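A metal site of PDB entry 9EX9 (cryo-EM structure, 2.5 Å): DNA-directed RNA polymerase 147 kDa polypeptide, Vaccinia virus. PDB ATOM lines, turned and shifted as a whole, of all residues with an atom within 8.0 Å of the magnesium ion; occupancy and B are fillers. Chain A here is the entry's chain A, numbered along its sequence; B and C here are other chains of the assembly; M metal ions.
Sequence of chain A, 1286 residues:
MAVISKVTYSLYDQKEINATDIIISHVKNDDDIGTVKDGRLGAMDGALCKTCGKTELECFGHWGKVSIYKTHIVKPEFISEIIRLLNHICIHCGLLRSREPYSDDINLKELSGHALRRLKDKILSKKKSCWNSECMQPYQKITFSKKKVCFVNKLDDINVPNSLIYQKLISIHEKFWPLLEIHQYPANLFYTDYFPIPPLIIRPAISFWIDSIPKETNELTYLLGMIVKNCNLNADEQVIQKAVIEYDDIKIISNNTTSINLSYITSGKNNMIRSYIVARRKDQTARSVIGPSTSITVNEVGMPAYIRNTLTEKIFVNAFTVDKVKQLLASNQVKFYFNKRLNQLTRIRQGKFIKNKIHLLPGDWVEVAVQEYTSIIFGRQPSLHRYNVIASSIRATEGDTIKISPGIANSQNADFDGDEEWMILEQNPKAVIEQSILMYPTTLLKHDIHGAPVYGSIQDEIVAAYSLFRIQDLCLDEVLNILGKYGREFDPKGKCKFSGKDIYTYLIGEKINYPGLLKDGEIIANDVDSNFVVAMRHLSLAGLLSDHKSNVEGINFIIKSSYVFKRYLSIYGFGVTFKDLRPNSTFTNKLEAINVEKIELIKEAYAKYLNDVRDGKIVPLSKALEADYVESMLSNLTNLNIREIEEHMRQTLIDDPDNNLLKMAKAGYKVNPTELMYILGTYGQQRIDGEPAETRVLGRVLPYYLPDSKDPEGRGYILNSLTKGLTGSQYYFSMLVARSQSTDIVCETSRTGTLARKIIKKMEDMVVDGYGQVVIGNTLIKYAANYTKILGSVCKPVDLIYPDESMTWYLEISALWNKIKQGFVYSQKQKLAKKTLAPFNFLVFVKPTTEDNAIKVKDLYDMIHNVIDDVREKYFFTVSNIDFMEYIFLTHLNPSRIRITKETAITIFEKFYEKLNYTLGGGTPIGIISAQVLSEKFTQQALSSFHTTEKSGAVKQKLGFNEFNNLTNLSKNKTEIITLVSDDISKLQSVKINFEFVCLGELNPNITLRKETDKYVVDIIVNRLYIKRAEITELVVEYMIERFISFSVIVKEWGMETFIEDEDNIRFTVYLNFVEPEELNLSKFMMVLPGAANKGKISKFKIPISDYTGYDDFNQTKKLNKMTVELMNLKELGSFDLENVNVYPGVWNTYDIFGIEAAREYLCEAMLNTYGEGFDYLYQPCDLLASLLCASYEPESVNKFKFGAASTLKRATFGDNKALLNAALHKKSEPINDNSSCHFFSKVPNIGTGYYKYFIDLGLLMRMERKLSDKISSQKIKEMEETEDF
Of the 21 residues printed, 3 come within 4 Å of the magnesium ion.
The nearest printed residue that does not touch the magnesium ion is Asn 226 of chain B (4.3 Å).
The magnesium ion is bound by OD1 of Asp 417, 1.9 Å away.
OD1 of Asp 419 is bound to the magnesium ion (2.2 Å).
The magnesium ion is bound by the side-chain carboxylate (OD1) of Asp 415 (2.5 Å).
The magnesium ion has three donor atoms within binding distance.
Slightly farther from the magnesium ion lies the side-chain carboxylate (OD2) of Asp 417 (2.7 Å).
O of Asp 419 is in hydrogen-bond range of N of Ile 290, 3.4 Å away.
The guanidinium group (NE) of Arg 380 lies within salt-bridge range of the side-chain carboxylate (OD2) of Asp 419 (3.3 Å).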
ATOM      1  N   ILE A 290      17.573  -3.239 -12.511  1.00  0.00           N
ATOM      2  CA  ILE A 290      17.527  -4.468 -11.739  1.00  0.00           C
ATOM      3  C   ILE A 290      18.875  -5.170 -11.809  1.00  0.00           C
ATOM      4  O   ILE A 290      19.730  -4.867 -12.634  1.00  0.00           O
ATOM      5  CB  ILE A 290      16.401  -5.410 -12.207  1.00  0.00           C
ATOM      6  CG1 ILE A 290      16.565  -5.754 -13.685  1.00  0.00           C
ATOM      7  CG2 ILE A 290      15.042  -4.794 -11.941  1.00  0.00           C
ATOM      8  CD1 ILE A 290      15.607  -6.808 -14.162  1.00  0.00           C
ATOM      9  N   ARG A 380       7.733  -5.665 -14.501  1.00  0.00           N
ATOM     10  CA  ARG A 380       8.514  -5.260 -15.664  1.00  0.00           C
ATOM     11  C   ARG A 380       7.556  -4.992 -16.823  1.00  0.00           C
ATOM     12  O   ARG A 380       6.476  -5.582 -16.886  1.00  0.00           O
ATOM     13  CB  ARG A 380       9.515  -6.347 -16.060  1.00  0.00           C
ATOM     14  CG  ARG A 380      10.366  -6.007 -17.255  1.00  0.00           C
ATOM     15  CD  ARG A 380      11.389  -7.093 -17.534  1.00  0.00           C
ATOM     16  NE  ARG A 380      12.093  -6.858 -18.788  1.00  0.00           N
ATOM     17  CZ  ARG A 380      11.612  -7.127 -19.986  1.00  0.00           C
ATOM     18  NH1 ARG A 380      10.406  -7.663 -20.142  1.00  0.00           N
ATOM     19  NH2 ARG A 380      12.342  -6.873 -21.061  1.00  0.00           N
ATOM     20  N   ASN A 413      10.601 -12.428 -18.630  1.00  0.00           N
ATOM     21  CA  ASN A 413      11.369 -12.208 -19.860  1.00  0.00           C
ATOM     22  C   ASN A 413      12.459 -11.161 -19.642  1.00  0.00           C
ATOM     23  O   ASN A 413      12.759 -10.360 -20.516  1.00  0.00           O
ATOM     24  CB  ASN A 413      10.443 -11.799 -21.007  1.00  0.00           C
ATOM     25  CG  ASN A 413      11.154 -11.782 -22.343  1.00  0.00           C
ATOM     26  OD1 ASN A 413      12.196 -12.406 -22.517  1.00  0.00           O
ATOM     27  ND2 ASN A 413      10.590 -11.049 -23.295  1.00  0.00           N
ATOM     28  N   ALA A 414      13.079 -11.197 -18.463  1.00  0.00           N
ATOM     29  CA  ALA A 414      14.027 -10.189 -18.041  1.00  0.00           C
ATOM     30  C   ALA A 414      15.450 -10.727 -18.086  1.00  0.00           C
ATOM     31  O   ALA A 414      15.688 -11.933 -17.992  1.00  0.00           O
ATOM     32  CB  ALA A 414      13.714  -9.707 -16.628  1.00  0.00           C
ATOM     33  N   ASP A 415      16.407  -9.811 -18.239  1.00  0.00           N
ATOM     34  CA  ASP A 415      17.823 -10.111 -18.066  1.00  0.00           C
ATOM     35  C   ASP A 415      18.475  -8.872 -17.472  1.00  0.00           C
ATOM     36  O   ASP A 415      17.807  -7.886 -17.144  1.00  0.00           O
ATOM     37  CB  ASP A 415      18.447 -10.556 -19.389  1.00  0.00           C
ATOM     38  CG  ASP A 415      18.235  -9.554 -20.502  1.00  0.00           C
ATOM     39  OD1 ASP A 415      17.661  -8.484 -20.243  1.00  0.00           O
ATOM     40  OD2 ASP A 415      18.645  -9.851 -21.639  1.00  0.00           O
ATOM     41  N   PHE A 416      19.799  -8.905 -17.319  1.00  0.00           N
ATOM     42  CA  PHE A 416      20.526  -7.882 -16.583  1.00  0.00           C
ATOM     43  C   PHE A 416      21.513  -7.152 -17.474  1.00  0.00           C
ATOM     44  O   PHE A 416      22.639  -6.858 -17.084  1.00  0.00           O
ATOM     45  CB  PHE A 416      21.217  -8.490 -15.377  1.00  0.00           C
ATOM     46  CG  PHE A 416      20.320  -9.358 -14.543  1.00  0.00           C
ATOM     47  CD1 PHE A 416      19.238  -8.816 -13.886  1.00  0.00           C
ATOM     48  CD2 PHE A 416      20.563 -10.711 -14.427  1.00  0.00           C
ATOM     49  CE1 PHE A 416      18.409  -9.609 -13.122  1.00  0.00           C
ATOM     50  CE2 PHE A 416      19.727 -11.504 -13.671  1.00  0.00           C
ATOM     51  CZ  PHE A 416      18.655 -10.944 -13.024  1.00  0.00           C
ATOM     52  N   ASP A 417      21.093  -6.844 -18.700  1.00  0.00           N
ATOM     53  CA  ASP A 417      21.886  -6.047 -19.622  1.00  0.00           C
ATOM     54  C   ASP A 417      21.437  -4.592 -19.665  1.00  0.00           C
ATOM     55  O   ASP A 417      21.821  -3.850 -20.570  1.00  0.00           O
ATOM     56  CB  ASP A 417      21.833  -6.643 -21.026  1.00  0.00           C
ATOM     57  CG  ASP A 417      20.438  -6.646 -21.616  1.00  0.00           C
ATOM     58  OD1 ASP A 417      19.491  -6.187 -20.952  1.00  0.00           O
ATOM     59  OD2 ASP A 417      20.276  -7.106 -22.765  1.00  0.00           O
ATOM     60  N   GLY A 418      20.606  -4.175 -18.708  1.00  0.00           N
ATOM     61  CA  GLY A 418      20.143  -2.802 -18.662  1.00  0.00           C
ATOM     62  C   GLY A 418      18.642  -2.670 -18.466  1.00  0.00           C
ATOM     63  O   GLY A 418      18.101  -1.577 -18.596  1.00  0.00           O
ATOM     64  N   ASP A 419      17.980  -3.771 -18.146  1.00  0.00           N
ATOM     65  CA  ASP A 419      16.540  -3.731 -17.930  1.00  0.00           C
ATOM     66  C   ASP A 419      16.199  -2.948 -16.669  1.00  0.00           C
ATOM     67  O   ASP A 419      17.045  -2.738 -15.791  1.00  0.00           O
ATOM     68  CB  ASP A 419      15.973  -5.146 -17.834  1.00  0.00           C
ATOM     69  CG  ASP A 419      16.161  -5.943 -19.088  1.00  0.00           C
ATOM     70  OD1 ASP A 419      17.111  -5.665 -19.849  1.00  0.00           O
ATOM     71  OD2 ASP A 419      15.339  -6.847 -19.350  1.00  0.00           O
ATOM     72  N   GLU A 420      14.950  -2.508 -16.586  1.00  0.00           N
ATOM     73  CA  GLU A 420      14.447  -1.755 -15.445  1.00  0.00           C
ATOM     74  C   GLU A 420      13.113  -2.336 -14.998  1.00  0.00           C
ATOM     75  O   GLU A 420      12.437  -3.028 -15.757  1.00  0.00           O
ATOM     76  CB  GLU A 420      14.265  -0.277 -15.794  1.00  0.00           C
ATOM     77  CG  GLU A 420      15.550   0.431 -16.166  1.00  0.00           C
ATOM     78  CD  GLU A 420      15.315   1.886 -16.504  1.00  0.00           C
ATOM     79  OE1 GLU A 420      14.185   2.373 -16.303  1.00  0.00           O
ATOM     80  OE2 GLU A 420      16.258   2.541 -16.991  1.00  0.00           O
ATOM     81  N   PRO B 223      12.635 -14.069 -26.791  1.00  0.00           N
ATOM     82  CA  PRO B 223      13.706 -13.336 -27.487  1.00  0.00           C
ATOM     83  C   PRO B 223      14.922 -13.138 -26.584  1.00  0.00           C
ATOM     84  O   PRO B 223      14.797 -12.870 -25.395  1.00  0.00           O
ATOM     85  CB  PRO B 223      13.049 -11.998 -27.845  1.00  0.00           C
ATOM     86  CG  PRO B 223      11.600 -12.292 -27.879  1.00  0.00           C
ATOM     87  CD  PRO B 223      11.358 -13.331 -26.846  1.00  0.00           C
ATOM     88  N   ASP B 224      16.102 -13.262 -27.193  1.00  0.00           N
ATOM     89  CA  ASP B 224      17.349 -13.103 -26.438  1.00  0.00           C
ATOM     90  C   ASP B 224      17.666 -11.639 -26.182  1.00  0.00           C
ATOM     91  O   ASP B 224      18.214 -11.300 -25.121  1.00  0.00           O
ATOM     92  CB  ASP B 224      18.506 -13.757 -27.197  1.00  0.00           C
ATOM     93  CG  ASP B 224      19.844 -13.545 -26.519  1.00  0.00           C
ATOM     94  OD1 ASP B 224      20.027 -14.056 -25.396  1.00  0.00           O
ATOM     95  OD2 ASP B 224      20.718 -12.871 -27.094  1.00  0.00           O
ATOM     96  N   ASN B 225      17.325 -10.754 -27.109  1.00  0.00           N
ATOM     97  CA  ASN B 225      17.639  -9.335 -27.024  1.00  0.00           C
ATOM     98  C   ASN B 225      16.352  -8.529 -27.062  1.00  0.00           C
ATOM     99  O   ASN B 225      15.448  -8.826 -27.851  1.00  0.00           O
ATOM    100  CB  ASN B 225      18.577  -8.912 -28.157  1.00  0.00           C
ATOM    101  CG  ASN B 225      19.076  -7.492 -28.025  1.00  0.00           C
ATOM    102  OD1 ASN B 225      20.083  -7.232 -27.371  1.00  0.00           O
ATOM    103  ND2 ASN B 225      18.376  -6.560 -28.663  1.00  0.00           N
ATOM    104  N   ASN B 226      16.264  -7.517 -26.209  1.00  0.00           N
ATOM    105  CA  ASN B 226      15.121  -6.622 -26.170  1.00  0.00           C
ATOM    106  C   ASN B 226      15.617  -5.175 -26.148  1.00  0.00           C
ATOM    107  O   ASN B 226      16.715  -4.902 -25.675  1.00  0.00           O
ATOM    108  CB  ASN B 226      14.240  -6.883 -24.941  1.00  0.00           C
ATOM    109  CG  ASN B 226      13.495  -8.185 -25.032  1.00  0.00           C
ATOM    110  OD1 ASN B 226      12.366  -8.240 -25.508  1.00  0.00           O
ATOM    111  ND2 ASN B 226      14.129  -9.260 -24.579  1.00  0.00           N
ATOM    112  N   PRO B 227      14.800  -4.232 -26.650  1.00  0.00           N
ATOM    113  CA  PRO B 227      15.228  -2.833 -26.711  1.00  0.00           C
ATOM    114  C   PRO B 227      15.380  -2.193 -25.335  1.00  0.00           C
ATOM    115  O   PRO B 227      14.491  -2.316 -24.494  1.00  0.00           O
ATOM    116  CB  PRO B 227      14.105  -2.163 -27.491  1.00  0.00           C
ATOM    117  CG  PRO B 227      12.915  -3.008 -27.265  1.00  0.00           C
ATOM    118  CD  PRO B 227      13.431  -4.409 -27.166  1.00  0.00           C
ATOM    119  N   SEP B 228      16.503  -1.519 -25.114  1.00  0.00           N
ATOM    120  CA  SEP B 228      16.766  -0.829 -23.859  1.00  0.00           C
ATOM    121  CB  SEP B 228      18.069  -0.057 -23.939  1.00  0.00           C
ATOM    122  OG  SEP B 228      19.157  -0.929 -24.190  1.00  0.00           O
ATOM    123  C   SEP B 228      15.612   0.107 -23.526  1.00  0.00           C
ATOM    124  O   SEP B 228      14.917   0.580 -24.415  1.00  0.00           O
ATOM    125  P   SEP B 228      20.083  -0.396 -25.390  1.00  0.00           P
ATOM    126  O1P SEP B 228      19.493  -0.916 -26.793  1.00  0.00           O
ATOM    127  O2P SEP B 228      20.158   1.208 -25.386  1.00  0.00           O
ATOM    128  O3P SEP B 228      21.572  -0.990 -25.203  1.00  0.00           O
ATOM    129  N   PRO B 229      15.405   0.393 -22.222  1.00  0.00           N
ATOM    130  CA  PRO B 229      14.309   1.284 -21.842  1.00  0.00           C
ATOM    131  C   PRO B 229      14.467   2.695 -22.433  1.00  0.00           C
ATOM    132  O   PRO B 229      15.595   3.178 -22.529  1.00  0.00           O
ATOM    133  CB  PRO B 229      14.391   1.325 -20.320  1.00  0.00           C
ATOM    134  CG  PRO B 229      15.162   0.112 -19.941  1.00  0.00           C
ATOM    135  CD  PRO B 229      16.129  -0.109 -21.042  1.00  0.00           C
ATOM    136  N   GLU C 755      23.105 -13.994 -16.979  1.00  0.00           N
ATOM    137  CA  GLU C 755      22.272 -13.134 -17.829  1.00  0.00           C
ATOM    138  C   GLU C 755      22.927 -11.773 -18.057  1.00  0.00           C
ATOM    139  O   GLU C 755      22.277 -10.728 -17.984  1.00  0.00           O
ATOM    140  CB  GLU C 755      20.878 -12.976 -17.229  1.00  0.00           C
ATOM    141  CG  GLU C 755      20.112 -14.269 -17.041  1.00  0.00           C
ATOM    142  CD  GLU C 755      19.624 -14.865 -18.341  1.00  0.00           C
ATOM    143  OE1 GLU C 755      19.208 -14.094 -19.228  1.00  0.00           O
ATOM    144  OE2 GLU C 755      19.658 -16.110 -18.478  1.00  0.00           O
ATOM    145  N   ASP C 756      24.225 -11.800 -18.361  1.00  0.00           N
ATOM    146  CA  ASP C 756      25.032 -10.649 -18.752  1.00  0.00           C
ATOM    147  C   ASP C 756      25.535  -9.817 -17.584  1.00  0.00           C
ATOM    148  O   ASP C 756      26.176  -8.798 -17.823  1.00  0.00           O
ATOM    149  CB  ASP C 756      24.289  -9.707 -19.708  1.00  0.00           C
ATOM    150  CG  ASP C 756      23.698 -10.434 -20.899  1.00  0.00           C
ATOM    151  OD1 ASP C 756      24.397 -11.292 -21.473  1.00  0.00           O
ATOM    152  OD2 ASP C 756      22.548 -10.130 -21.266  1.00  0.00           O
ATOM    153  N   LYS C 882      27.222   0.150 -16.789  1.00  0.00           N
ATOM    154  CA  LYS C 882      27.167  -0.621 -18.025  1.00  0.00           C
ATOM    155  C   LYS C 882      28.517  -0.591 -18.738  1.00  0.00           C
ATOM    156  O   LYS C 882      29.112   0.479 -18.897  1.00  0.00           O
ATOM    157  CB  LYS C 882      26.078  -0.046 -18.939  1.00  0.00           C
ATOM    158  CG  LYS C 882      25.421  -1.043 -19.852  1.00  0.00           C
ATOM    159  CD  LYS C 882      24.242  -0.399 -20.565  1.00  0.00           C
ATOM    160  CE  LYS C 882      23.685  -1.309 -21.635  1.00  0.00           C
ATOM    161  NZ  LYS C 882      22.559  -0.666 -22.356  1.00  0.00           N
ATOM    162  N   LYS C 890      27.778  -6.785 -23.954  1.00  0.00           N
ATOM    163  CA  LYS C 890      27.449  -5.748 -22.988  1.00  0.00           C
ATOM    164  C   LYS C 890      26.902  -6.370 -21.708  1.00  0.00           C
ATOM    165  O   LYS C 890      26.206  -7.375 -21.735  1.00  0.00           O
ATOM    166  CB  LYS C 890      26.427  -4.764 -23.563  1.00  0.00           C
ATOM    167  CG  LYS C 890      25.133  -5.407 -23.984  1.00  0.00           C
ATOM    168  CD  LYS C 890      24.101  -4.379 -24.402  1.00  0.00           C
ATOM    169  CE  LYS C 890      22.817  -5.046 -24.843  1.00  0.00           C
ATOM    170  NZ  LYS C 890      21.762  -4.072 -25.209  1.00  0.00           N
HETATM  171 MG    MG M   1      17.816  -6.445 -21.765  1.00  0.00          MG
